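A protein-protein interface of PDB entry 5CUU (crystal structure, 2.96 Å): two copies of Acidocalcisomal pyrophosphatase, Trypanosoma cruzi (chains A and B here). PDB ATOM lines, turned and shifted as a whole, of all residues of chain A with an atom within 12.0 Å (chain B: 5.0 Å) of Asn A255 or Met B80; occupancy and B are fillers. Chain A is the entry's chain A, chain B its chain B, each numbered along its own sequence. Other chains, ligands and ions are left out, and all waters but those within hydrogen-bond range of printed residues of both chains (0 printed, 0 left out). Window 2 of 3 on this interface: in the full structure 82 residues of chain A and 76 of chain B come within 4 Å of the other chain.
The side-chain carboxylate of Glu B76 sits at hydrogen-bond distance from the side-chain amide nitrogen of Asn A255 (2.6 Å).
The indole nitrogen (NE1) of Trp B139 is in hydrogen-bond range of the side-chain amide oxygen (OD1) of Asn A255, at 3.2 Å.
O of Lys A254 sits close to OE2 of Glu B76, at 3.4 Å.
Printed residues of chain A that touch a printed residue of chain B: Lys A254, Asn A255, Gly A256 and Val A257.
Hydrophobic or aromatic side chains of chain A within 4 Å of the printed part of chain B: Val A257.
Of the 15 printed residues of chain B, 5 touch a printed residue of chain A.
Among the printed residues, no Asp or Glu carboxylate lies within 4 Å of a Lys or Arg side-chain nitrogen of the other chain.
CB of Asn A255 touches CE of Met B80 (3.6 Å).
Gly A256 touches Val B79.
Gly A256 touches Leu B107.
Val A257 touches Glu B76 (CG2 to CG, 3.3 Å).
No position is printed for both chains.
Asn A255 touches just these residues of chain B: Glu B76, Met B80 and Trp B139.
Printed residues of chain A within 4 Å of Met B80: Asn A255.
Glu B76 touches just these residues of chain A: Lys A254, Asn A255 and Val A257.
No residue of chain A comes within 4 Å of Lys B77.
Of chain A, only Gly A256 comes within 4 Å of Val B79.
No residue of chain A comes within 4 Å of Arg B82.
Of chain A, only Gly A256 (3.5 Å) comes within 4 Å of Leu B107.
No residue of chain A comes within 4 Å of Trp B136.
Of the printed residues of chain A, Trp B139 touches Asn A255.
Printed residues of chain B within 4 Å of Lys A254: Glu B76 (3.4 Å).
Of the printed residues of chain B, Val A257 touches Glu B76 (3.3 Å).
Printed residues of chain B within 4 Å of Gly A256: Val B79 and Leu B107.
The nearest residue of chain A that does not touch Met B80 is Gly A256 (4.7 Å).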
ATOM      1  N   TYR A 177      15.541   0.636 -25.375  1.00  0.00           N
ATOM      2  CA  TYR A 177      16.813   1.217 -25.791  1.00  0.00           C
ATOM      3  C   TYR A 177      16.803   2.728 -25.513  1.00  0.00           C
ATOM      4  O   TYR A 177      17.314   3.517 -26.324  1.00  0.00           O
ATOM      5  CB  TYR A 177      17.078   0.972 -27.292  1.00  0.00           C
ATOM      6  CG  TYR A 177      17.192  -0.488 -27.704  1.00  0.00           C
ATOM      7  CD1 TYR A 177      18.291  -1.258 -27.319  1.00  0.00           C
ATOM      8  CD2 TYR A 177      16.151  -1.116 -28.404  1.00  0.00           C
ATOM      9  CE1 TYR A 177      18.348  -2.627 -27.601  1.00  0.00           C
ATOM     10  CE2 TYR A 177      16.190  -2.482 -28.693  1.00  0.00           C
ATOM     11  CZ  TYR A 177      17.287  -3.241 -28.280  1.00  0.00           C
ATOM     12  OH  TYR A 177      17.285  -4.612 -28.465  1.00  0.00           O
ATOM     13  N   THR A 178      16.213   3.099 -24.364  1.00  0.00           N
ATOM     14  CA  THR A 178      16.074   4.492 -23.880  1.00  0.00           C
ATOM     15  C   THR A 178      15.939   4.489 -22.350  1.00  0.00           C
ATOM     16  O   THR A 178      15.516   3.492 -21.767  1.00  0.00           O
ATOM     17  CB  THR A 178      14.798   5.208 -24.446  1.00  0.00           C
ATOM     18  OG1 THR A 178      13.653   4.895 -23.632  1.00  0.00           O
ATOM     19  CG2 THR A 178      14.536   4.790 -25.896  1.00  0.00           C
ATOM     20  N   PRO A 179      16.241   5.621 -21.683  1.00  0.00           N
ATOM     21  CA  PRO A 179      16.149   5.691 -20.216  1.00  0.00           C
ATOM     22  C   PRO A 179      14.770   5.528 -19.572  1.00  0.00           C
ATOM     23  O   PRO A 179      14.658   5.513 -18.348  1.00  0.00           O
ATOM     24  CB  PRO A 179      16.739   7.060 -19.891  1.00  0.00           C
ATOM     25  CG  PRO A 179      17.514   7.441 -21.119  1.00  0.00           C
ATOM     26  CD  PRO A 179      16.714   6.900 -22.241  1.00  0.00           C
ATOM     27  N   SER A 180      13.719   5.401 -20.374  1.00  0.00           N
ATOM     28  CA  SER A 180      12.366   5.306 -19.819  1.00  0.00           C
ATOM     29  C   SER A 180      11.836   3.904 -19.645  1.00  0.00           C
ATOM     30  O   SER A 180      10.955   3.675 -18.813  1.00  0.00           O
ATOM     31  CB  SER A 180      11.371   6.099 -20.687  1.00  0.00           C
ATOM     32  OG  SER A 180      11.155   5.504 -21.963  1.00  0.00           O
ATOM     33  N   ARG A 182      11.087   0.456 -18.534  1.00  0.00           N
ATOM     34  CA  ARG A 182      11.128  -0.224 -17.263  1.00  0.00           C
ATOM     35  C   ARG A 182      10.282  -1.468 -17.390  1.00  0.00           C
ATOM     36  O   ARG A 182       9.505  -1.638 -18.325  1.00  0.00           O
ATOM     37  CB  ARG A 182      10.546   0.648 -16.154  1.00  0.00           C
ATOM     38  CG  ARG A 182      11.406   1.839 -15.779  1.00  0.00           C
ATOM     39  CD  ARG A 182      12.684   1.414 -15.064  1.00  0.00           C
ATOM     40  NE  ARG A 182      13.481   2.564 -14.694  1.00  0.00           N
ATOM     41  CZ  ARG A 182      13.997   3.416 -15.569  1.00  0.00           C
ATOM     42  NH1 ARG A 182      13.809   3.239 -16.865  1.00  0.00           N
ATOM     43  NH2 ARG A 182      14.676   4.462 -15.139  1.00  0.00           N
ATOM     44  N   GLU A 239      18.910  -4.670 -15.788  1.00  0.00           N
ATOM     45  CA  GLU A 239      19.204  -4.944 -14.390  1.00  0.00           C
ATOM     46  C   GLU A 239      18.118  -4.530 -13.433  1.00  0.00           C
ATOM     47  O   GLU A 239      17.416  -3.565 -13.668  1.00  0.00           O
ATOM     48  CB  GLU A 239      20.445  -4.214 -14.008  1.00  0.00           C
ATOM     49  CG  GLU A 239      20.278  -2.756 -14.277  1.00  0.00           C
ATOM     50  CD  GLU A 239      21.595  -2.083 -14.319  1.00  0.00           C
ATOM     51  OE1 GLU A 239      22.263  -2.079 -13.254  1.00  0.00           O
ATOM     52  OE2 GLU A 239      21.960  -1.594 -15.413  1.00  0.00           O
ATOM     53  N   LYS A 250      15.440  -1.997 -15.248  1.00  0.00           N
ATOM     54  CA  LYS A 250      15.651  -0.868 -16.122  1.00  0.00           C
ATOM     55  C   LYS A 250      16.784  -1.254 -17.019  1.00  0.00           C
ATOM     56  O   LYS A 250      17.398  -2.274 -16.809  1.00  0.00           O
ATOM     57  CB  LYS A 250      16.010   0.378 -15.306  1.00  0.00           C
ATOM     58  CG  LYS A 250      17.251   0.209 -14.441  1.00  0.00           C
ATOM     59  CD  LYS A 250      18.460   0.933 -14.999  1.00  0.00           C
ATOM     60  CE  LYS A 250      18.516   2.336 -14.459  1.00  0.00           C
ATOM     61  NZ  LYS A 250      18.683   2.366 -12.968  1.00  0.00           N
ATOM     62  N   GLN A 251      17.064  -0.449 -18.022  1.00  0.00           N
ATOM     63  CA  GLN A 251      18.154  -0.776 -18.915  1.00  0.00           C
ATOM     64  C   GLN A 251      19.443  -0.062 -18.496  1.00  0.00           C
ATOM     65  O   GLN A 251      19.411   0.952 -17.797  1.00  0.00           O
ATOM     66  CB  GLN A 251      17.771  -0.404 -20.348  1.00  0.00           C
ATOM     67  CG  GLN A 251      18.397  -1.305 -21.386  1.00  0.00           C
ATOM     68  CD  GLN A 251      17.802  -1.074 -22.743  1.00  0.00           C
ATOM     69  OE1 GLN A 251      16.627  -0.698 -22.863  1.00  0.00           O
ATOM     70  NE2 GLN A 251      18.604  -1.308 -23.787  1.00  0.00           N
ATOM     71  N   ASP A 252      20.577  -0.608 -18.910  1.00  0.00           N
ATOM     72  CA  ASP A 252      21.849  -0.010 -18.576  1.00  0.00           C
ATOM     73  C   ASP A 252      22.075   1.056 -19.629  1.00  0.00           C
ATOM     74  O   ASP A 252      22.316   0.760 -20.789  1.00  0.00           O
ATOM     75  CB  ASP A 252      22.959  -1.077 -18.605  1.00  0.00           C
ATOM     76  CG  ASP A 252      24.177  -0.723 -17.715  1.00  0.00           C
ATOM     77  OD1 ASP A 252      24.009  -0.478 -16.502  1.00  0.00           O
ATOM     78  OD2 ASP A 252      25.325  -0.719 -18.227  1.00  0.00           O
ATOM     79  N   ILE A 253      21.933   2.305 -19.211  1.00  0.00           N
ATOM     80  CA  ILE A 253      22.141   3.465 -20.072  1.00  0.00           C
ATOM     81  C   ILE A 253      23.117   4.366 -19.307  1.00  0.00           C
ATOM     82  O   ILE A 253      22.945   4.625 -18.111  1.00  0.00           O
ATOM     83  CB  ILE A 253      20.847   4.293 -20.299  1.00  0.00           C
ATOM     84  CG1 ILE A 253      19.608   3.391 -20.403  1.00  0.00           C
ATOM     85  CG2 ILE A 253      21.011   5.136 -21.538  1.00  0.00           C
ATOM     86  CD1 ILE A 253      19.465   2.595 -21.693  1.00  0.00           C
ATOM     87  N   LYS A 254      24.163   4.806 -19.993  1.00  0.00           N
ATOM     88  CA  LYS A 254      25.149   5.704 -19.415  1.00  0.00           C
ATOM     89  C   LYS A 254      25.220   6.844 -20.427  1.00  0.00           C
ATOM     90  O   LYS A 254      25.442   6.615 -21.630  1.00  0.00           O
ATOM     91  CB  LYS A 254      26.505   4.998 -19.280  1.00  0.00           C
ATOM     92  CG  LYS A 254      27.690   5.938 -18.955  1.00  0.00           C
ATOM     93  CD  LYS A 254      29.085   5.234 -18.980  1.00  0.00           C
ATOM     94  CE  LYS A 254      29.390   4.453 -17.689  1.00  0.00           C
ATOM     95  NZ  LYS A 254      30.691   3.726 -17.755  1.00  0.00           N
ATOM     96  N   ASN A 255      25.002   8.065 -19.948  1.00  0.00           N
ATOM     97  CA  ASN A 255      25.023   9.251 -20.810  1.00  0.00           C
ATOM     98  C   ASN A 255      24.048   9.071 -21.977  1.00  0.00           C
ATOM     99  O   ASN A 255      24.422   9.240 -23.137  1.00  0.00           O
ATOM    100  CB  ASN A 255      26.426   9.538 -21.411  1.00  0.00           C
ATOM    101  CG  ASN A 255      27.584   9.276 -20.438  1.00  0.00           C
ATOM    102  OD1 ASN A 255      27.582   9.737 -19.297  1.00  0.00           O
ATOM    103  ND2 ASN A 255      28.591   8.544 -20.910  1.00  0.00           N
ATOM    104  N   GLY A 256      22.813   8.698 -21.666  1.00  0.00           N
ATOM    105  CA  GLY A 256      21.806   8.541 -22.699  1.00  0.00           C
ATOM    106  C   GLY A 256      21.922   7.413 -23.709  1.00  0.00           C
ATOM    107  O   GLY A 256      20.998   7.226 -24.506  1.00  0.00           O
ATOM    108  N   VAL A 257      23.020   6.660 -23.701  1.00  0.00           N
ATOM    109  CA  VAL A 257      23.181   5.558 -24.654  1.00  0.00           C
ATOM    110  C   VAL A 257      23.082   4.197 -23.969  1.00  0.00           C
ATOM    111  O   VAL A 257      23.700   3.975 -22.931  1.00  0.00           O
ATOM    112  CB  VAL A 257      24.543   5.619 -25.343  1.00  0.00           C
ATOM    113  CG1 VAL A 257      24.486   4.870 -26.667  1.00  0.00           C
ATOM    114  CG2 VAL A 257      24.968   7.070 -25.524  1.00  0.00           C
ATOM    115  N   PRO A 258      22.296   3.264 -24.530  1.00  0.00           N
ATOM    116  CA  PRO A 258      22.240   1.976 -23.837  1.00  0.00           C
ATOM    117  C   PRO A 258      23.570   1.203 -23.900  1.00  0.00           C
ATOM    118  O   PRO A 258      24.373   1.415 -24.810  1.00  0.00           O
ATOM    119  CB  PRO A 258      21.062   1.254 -24.531  1.00  0.00           C
ATOM    120  CG  PRO A 258      20.976   1.876 -25.846  1.00  0.00           C
ATOM    121  CD  PRO A 258      21.256   3.335 -25.566  1.00  0.00           C
ATOM    122  N   ARG A 259      23.805   0.333 -22.914  1.00  0.00           N
ATOM    123  CA  ARG A 259      25.030  -0.475 -22.849  1.00  0.00           C
ATOM    124  C   ARG A 259      24.807  -1.907 -23.367  1.00  0.00           C
ATOM    125  O   ARG A 259      23.706  -2.440 -23.286  1.00  0.00           O
ATOM    126  CB  ARG A 259      25.584  -0.495 -21.414  1.00  0.00           C
ATOM    127  CG  ARG A 259      26.119   0.853 -20.936  1.00  0.00           C
ATOM    128  CD  ARG A 259      27.077   1.423 -21.963  1.00  0.00           C
ATOM    129  NE  ARG A 259      28.212   2.117 -21.362  1.00  0.00           N
ATOM    130  CZ  ARG A 259      29.428   2.189 -21.918  1.00  0.00           C
ATOM    131  NH1 ARG A 259      30.413   2.846 -21.299  1.00  0.00           N
ATOM    132  NH2 ARG A 259      29.674   1.596 -23.092  1.00  0.00           N
ATOM    133  N   PHE A 260      25.865  -2.505 -23.902  1.00  0.00           N
ATOM    134  CA  PHE A 260      25.844  -3.846 -24.485  1.00  0.00           C
ATOM    135  C   PHE A 260      27.120  -4.637 -24.198  1.00  0.00           C
ATOM    136  O   PHE A 260      28.204  -4.074 -24.238  1.00  0.00           O
ATOM    137  CB  PHE A 260      25.760  -3.733 -25.991  1.00  0.00           C
ATOM    138  CG  PHE A 260      24.521  -3.110 -26.480  1.00  0.00           C
ATOM    139  CD1 PHE A 260      23.369  -3.868 -26.639  1.00  0.00           C
ATOM    140  CD2 PHE A 260      24.516  -1.798 -26.883  1.00  0.00           C
ATOM    141  CE1 PHE A 260      22.220  -3.335 -27.211  1.00  0.00           C
ATOM    142  CE2 PHE A 260      23.376  -1.253 -27.455  1.00  0.00           C
ATOM    143  CZ  PHE A 260      22.213  -2.032 -27.626  1.00  0.00           C
ATOM    144  N   LYS A 262      30.177  -6.182 -25.102  1.00  0.00           N
ATOM    145  CA  LYS A 262      30.835  -6.080 -26.415  1.00  0.00           C
ATOM    146  C   LYS A 262      31.570  -7.333 -26.786  1.00  0.00           C
ATOM    147  O   LYS A 262      31.848  -7.571 -27.945  1.00  0.00           O
ATOM    148  CB  LYS A 262      31.789  -4.872 -26.483  1.00  0.00           C
ATOM    149  CG  LYS A 262      31.078  -3.508 -26.546  1.00  0.00           C
ATOM    150  CD  LYS A 262      29.923  -3.538 -27.561  1.00  0.00           C
ATOM    151  CE  LYS A 262      29.920  -2.330 -28.508  1.00  0.00           C
ATOM    152  NZ  LYS A 262      29.817  -1.004 -27.860  1.00  0.00           N
ATOM    153  N   GLU B  76      27.801   9.525 -28.236  1.00  0.00           N
ATOM    154  CA  GLU B  76      26.878   9.938 -27.182  1.00  0.00           C
ATOM    155  C   GLU B  76      26.511  11.402 -27.399  1.00  0.00           C
ATOM    156  O   GLU B  76      25.361  11.793 -27.223  1.00  0.00           O
ATOM    157  CB  GLU B  76      27.528   9.784 -25.804  1.00  0.00           C
ATOM    158  CG  GLU B  76      27.995   8.380 -25.478  1.00  0.00           C
ATOM    159  CD  GLU B  76      28.749   8.305 -24.165  1.00  0.00           C
ATOM    160  OE1 GLU B  76      29.769   9.022 -24.023  1.00  0.00           O
ATOM    161  OE2 GLU B  76      28.321   7.525 -23.282  1.00  0.00           O
ATOM    162  N   LYS B  77      27.505  12.201 -27.787  1.00  0.00           N
ATOM    163  CA  LYS B  77      27.333  13.635 -28.033  1.00  0.00           C
ATOM    164  C   LYS B  77      26.074  13.981 -28.829  1.00  0.00           C
ATOM    165  O   LYS B  77      25.274  14.800 -28.389  1.00  0.00           O
ATOM    166  CB  LYS B  77      28.582  14.195 -28.740  1.00  0.00           C
ATOM    167  CG  LYS B  77      28.572  15.702 -28.959  1.00  0.00           C
ATOM    168  CD  LYS B  77      29.986  16.289 -29.002  1.00  0.00           C
ATOM    169  CE  LYS B  77      29.954  17.805 -29.217  1.00  0.00           C
ATOM    170  NZ  LYS B  77      29.003  18.515 -28.302  1.00  0.00           N
ATOM    171  N   ARG B  78      25.887  13.360 -29.990  1.00  0.00           N
ATOM    172  CA  ARG B  78      24.704  13.650 -30.800  1.00  0.00           C
ATOM    173  C   ARG B  78      23.420  13.136 -30.167  1.00  0.00           C
ATOM    174  O   ARG B  78      22.367  13.749 -30.342  1.00  0.00           O
ATOM    175  CB  ARG B  78      24.819  13.057 -32.207  1.00  0.00           C
ATOM    176  CG  ARG B  78      25.876  13.690 -33.111  1.00  0.00           C
ATOM    177  CD  ARG B  78      25.642  15.179 -33.424  1.00  0.00           C
ATOM    178  NE  ARG B  78      26.619  16.053 -32.771  1.00  0.00           N
ATOM    179  CZ  ARG B  78      27.917  15.773 -32.628  1.00  0.00           C
ATOM    180  NH1 ARG B  78      28.431  14.633 -33.083  1.00  0.00           N
ATOM    181  NH2 ARG B  78      28.715  16.644 -32.027  1.00  0.00           N
ATOM    182  N   VAL B  79      23.495  12.010 -29.454  1.00  0.00           N
ATOM    183  CA  VAL B  79      22.316  11.432 -28.785  1.00  0.00           C
ATOM    184  C   VAL B  79      21.962  12.256 -27.554  1.00  0.00           C
ATOM    185  O   VAL B  79      20.844  12.186 -27.034  1.00  0.00           O
ATOM    186  CB  VAL B  79      22.563   9.969 -28.343  1.00  0.00           C
ATOM    187  CG1 VAL B  79      21.534   9.549 -27.299  1.00  0.00           C
ATOM    188  CG2 VAL B  79      22.472   9.052 -29.547  1.00  0.00           C
ATOM    189  N   MET B  80      22.941  13.039 -27.109  1.00  0.00           N
ATOM    190  CA  MET B  80      22.821  13.917 -25.953  1.00  0.00           C
ATOM    191  C   MET B  80      22.299  15.273 -26.439  1.00  0.00           C
ATOM    192  O   MET B  80      21.622  15.989 -25.703  1.00  0.00           O
ATOM    193  CB  MET B  80      24.197  14.094 -25.304  1.00  0.00           C
ATOM    194  CG  MET B  80      24.145  14.531 -23.867  1.00  0.00           C
ATOM    195  SD  MET B  80      23.626  13.178 -22.806  1.00  0.00           S
ATOM    196  CE  MET B  80      25.172  12.829 -21.926  1.00  0.00           C
ATOM    197  N   ALA B  81      22.628  15.608 -27.686  1.00  0.00           N
ATOM    198  CA  ALA B  81      22.210  16.860 -28.312  1.00  0.00           C
ATOM    199  C   ALA B  81      20.738  16.788 -28.729  1.00  0.00           C
ATOM    200  O   ALA B  81      20.002  17.776 -28.619  1.00  0.00           O
ATOM    201  CB  ALA B  81      23.090  17.157 -29.532  1.00  0.00           C
ATOM    202  N   ARG B  82      20.314  15.617 -29.206  1.00  0.00           N
ATOM    203  CA  ARG B  82      18.929  15.411 -29.637  1.00  0.00           C
ATOM    204  C   ARG B  82      17.979  15.350 -28.444  1.00  0.00           C
ATOM    205  O   ARG B  82      16.820  15.743 -28.548  1.00  0.00           O
ATOM    206  CB  ARG B  82      18.795  14.122 -30.469  1.00  0.00           C
ATOM    207  CG  ARG B  82      19.521  14.140 -31.814  1.00  0.00           C
ATOM    208  CD  ARG B  82      18.970  13.087 -32.774  1.00  0.00           C
ATOM    209  NE  ARG B  82      19.018  11.727 -32.228  1.00  0.00           N
ATOM    210  CZ  ARG B  82      20.047  10.885 -32.340  1.00  0.00           C
ATOM    211  NH1 ARG B  82      21.154  11.242 -32.992  1.00  0.00           N
ATOM    212  NH2 ARG B  82      19.964   9.672 -31.799  1.00  0.00           N
ATOM    213  N   MET B  83      18.475  14.859 -27.311  1.00  0.00           N
ATOM    214  CA  MET B  83      17.657  14.760 -26.108  1.00  0.00           C
ATOM    215  C   MET B  83      17.502  16.134 -25.436  1.00  0.00           C
ATOM    216  O   MET B  83      16.523  16.377 -24.722  1.00  0.00           O
ATOM    217  CB  MET B  83      18.270  13.755 -25.124  1.00  0.00           C
ATOM    218  CG  MET B  83      17.237  13.140 -24.173  1.00  0.00           C
ATOM    219  SD  MET B  83      17.920  11.959 -22.979  1.00  0.00           S
ATOM    220  CE  MET B  83      18.312  10.542 -24.076  1.00  0.00           C
ATOM    221  N   PHE B  84      18.479  17.017 -25.666  1.00  0.00           N
ATOM    222  CA  PHE B  84      18.475  18.394 -25.135  1.00  0.00           C
ATOM    223  C   PHE B  84      17.429  19.189 -25.926  1.00  0.00           C
ATOM    224  O   PHE B  84      16.773  20.103 -25.398  1.00  0.00           O
ATOM    225  CB  PHE B  84      19.860  19.050 -25.320  1.00  0.00           C
ATOM    226  CG  PHE B  84      19.880  20.540 -25.043  1.00  0.00           C
ATOM    227  CD1 PHE B  84      19.976  21.023 -23.741  1.00  0.00           C
ATOM    228  CD2 PHE B  84      19.760  21.458 -26.092  1.00  0.00           C
ATOM    229  CE1 PHE B  84      19.950  22.395 -23.489  1.00  0.00           C
ATOM    230  CE2 PHE B  84      19.731  22.837 -25.851  1.00  0.00           C
ATOM    231  CZ  PHE B  84      19.825  23.305 -24.553  1.00  0.00           C
ATOM    232  N   MET B 103      16.094  16.770 -16.695  1.00  0.00           N
ATOM    233  CA  MET B 103      16.794  16.030 -17.747  1.00  0.00           C
ATOM    234  C   MET B 103      17.906  15.154 -17.170  1.00  0.00           C
ATOM    235  O   MET B 103      18.101  14.015 -17.605  1.00  0.00           O
ATOM    236  CB  MET B 103      17.379  16.978 -18.798  1.00  0.00           C
ATOM    237  CG  MET B 103      17.895  16.232 -20.020  1.00  0.00           C
ATOM    238  SD  MET B 103      18.445  17.285 -21.386  1.00  0.00           S
ATOM    239  CE  MET B 103      19.685  16.226 -22.229  1.00  0.00           C
ATOM    240  N   LEU B 107      18.357  11.233 -17.454  1.00  0.00           N
ATOM    241  CA  LEU B 107      19.545  10.491 -17.830  1.00  0.00           C
ATOM    242  C   LEU B 107      20.171   9.673 -16.688  1.00  0.00           C
ATOM    243  O   LEU B 107      21.388   9.461 -16.667  1.00  0.00           O
ATOM    244  CB  LEU B 107      20.581  11.451 -18.405  1.00  0.00           C
ATOM    245  CG  LEU B 107      20.241  12.092 -19.755  1.00  0.00           C
ATOM    246  CD1 LEU B 107      21.272  13.146 -20.138  1.00  0.00           C
ATOM    247  CD2 LEU B 107      20.202  11.012 -20.806  1.00  0.00           C
ATOM    248  N   PHE B 132      23.472  24.065 -24.985  1.00  0.00           N
ATOM    249  CA  PHE B 132      23.864  22.656 -24.989  1.00  0.00           C
ATOM    250  C   PHE B 132      25.379  22.538 -24.834  1.00  0.00           C
ATOM    251  O   PHE B 132      25.862  21.872 -23.915  1.00  0.00           O
ATOM    252  CB  PHE B 132      23.425  21.962 -26.294  1.00  0.00           C
ATOM    253  CG  PHE B 132      23.948  20.550 -26.436  1.00  0.00           C
ATOM    254  CD1 PHE B 132      23.664  19.586 -25.468  1.00  0.00           C
ATOM    255  CD2 PHE B 132      24.774  20.202 -27.503  1.00  0.00           C
ATOM    256  CE1 PHE B 132      24.201  18.303 -25.560  1.00  0.00           C
ATOM    257  CE2 PHE B 132      25.316  18.921 -27.604  1.00  0.00           C
ATOM    258  CZ  PHE B 132      25.030  17.972 -26.630  1.00  0.00           C
ATOM    259  N   PHE B 135      26.220  22.827 -21.530  1.00  0.00           N
ATOM    260  CA  PHE B 135      25.722  21.679 -20.778  1.00  0.00           C
ATOM    261  C   PHE B 135      26.596  20.428 -20.999  1.00  0.00           C
ATOM    262  O   PHE B 135      27.128  19.860 -20.040  1.00  0.00           O
ATOM    263  CB  PHE B 135      24.274  21.380 -21.182  1.00  0.00           C
ATOM    264  CG  PHE B 135      23.702  20.162 -20.512  1.00  0.00           C
ATOM    265  CD1 PHE B 135      23.671  20.068 -19.119  1.00  0.00           C
ATOM    266  CD2 PHE B 135      23.208  19.100 -21.273  1.00  0.00           C
ATOM    267  CE1 PHE B 135      23.154  18.928 -18.489  1.00  0.00           C
ATOM    268  CE2 PHE B 135      22.691  17.959 -20.659  1.00  0.00           C
ATOM    269  CZ  PHE B 135      22.663  17.870 -19.262  1.00  0.00           C
ATOM    270  N   TRP B 136      26.734  20.011 -22.260  1.00  0.00           N
ATOM    271  CA  TRP B 136      27.539  18.838 -22.628  1.00  0.00           C
ATOM    272  C   TRP B 136      28.926  18.912 -21.974  1.00  0.00           C
ATOM    273  O   TRP B 136      29.347  17.979 -21.280  1.00  0.00           O
ATOM    274  CB  TRP B 136      27.647  18.756 -24.167  1.00  0.00           C
ATOM    275  CG  TRP B 136      28.504  17.619 -24.764  1.00  0.00           C
ATOM    276  CD1 TRP B 136      29.541  17.765 -25.647  1.00  0.00           C
ATOM    277  CD2 TRP B 136      28.358  16.192 -24.560  1.00  0.00           C
ATOM    278  NE1 TRP B 136      30.047  16.534 -26.006  1.00  0.00           N
ATOM    279  CE2 TRP B 136      29.343  15.552 -25.355  1.00  0.00           C
ATOM    280  CE3 TRP B 136      27.497  15.399 -23.788  1.00  0.00           C
ATOM    281  CZ2 TRP B 136      29.489  14.157 -25.400  1.00  0.00           C
ATOM    282  CZ3 TRP B 136      27.644  14.012 -23.834  1.00  0.00           C
ATOM    283  CH2 TRP B 136      28.635  13.408 -24.638  1.00  0.00           C
ATOM    284  N   TRP B 139      28.708  18.267 -18.310  1.00  0.00           N
ATOM    285  CA  TRP B 139      28.356  16.866 -18.085  1.00  0.00           C
ATOM    286  C   TRP B 139      29.607  15.999 -18.126  1.00  0.00           C
ATOM    287  O   TRP B 139      29.980  15.351 -17.136  1.00  0.00           O
ATOM    288  CB  TRP B 139      27.360  16.417 -19.170  1.00  0.00           C
ATOM    289  CG  TRP B 139      26.793  15.032 -18.994  1.00  0.00           C
ATOM    290  CD1 TRP B 139      27.390  13.847 -19.322  1.00  0.00           C
ATOM    291  CD2 TRP B 139      25.524  14.697 -18.422  1.00  0.00           C
ATOM    292  NE1 TRP B 139      26.572  12.795 -18.988  1.00  0.00           N
ATOM    293  CE2 TRP B 139      25.419  13.288 -18.433  1.00  0.00           C
ATOM    294  CE3 TRP B 139      24.462  15.451 -17.899  1.00  0.00           C
ATOM    295  CZ2 TRP B 139      24.296  12.616 -17.941  1.00  0.00           C
ATOM    296  CZ3 TRP B 139      23.346  14.789 -17.412  1.00  0.00           C
ATOM    297  CH2 TRP B 139      23.272  13.383 -17.435  1.00  0.00           C
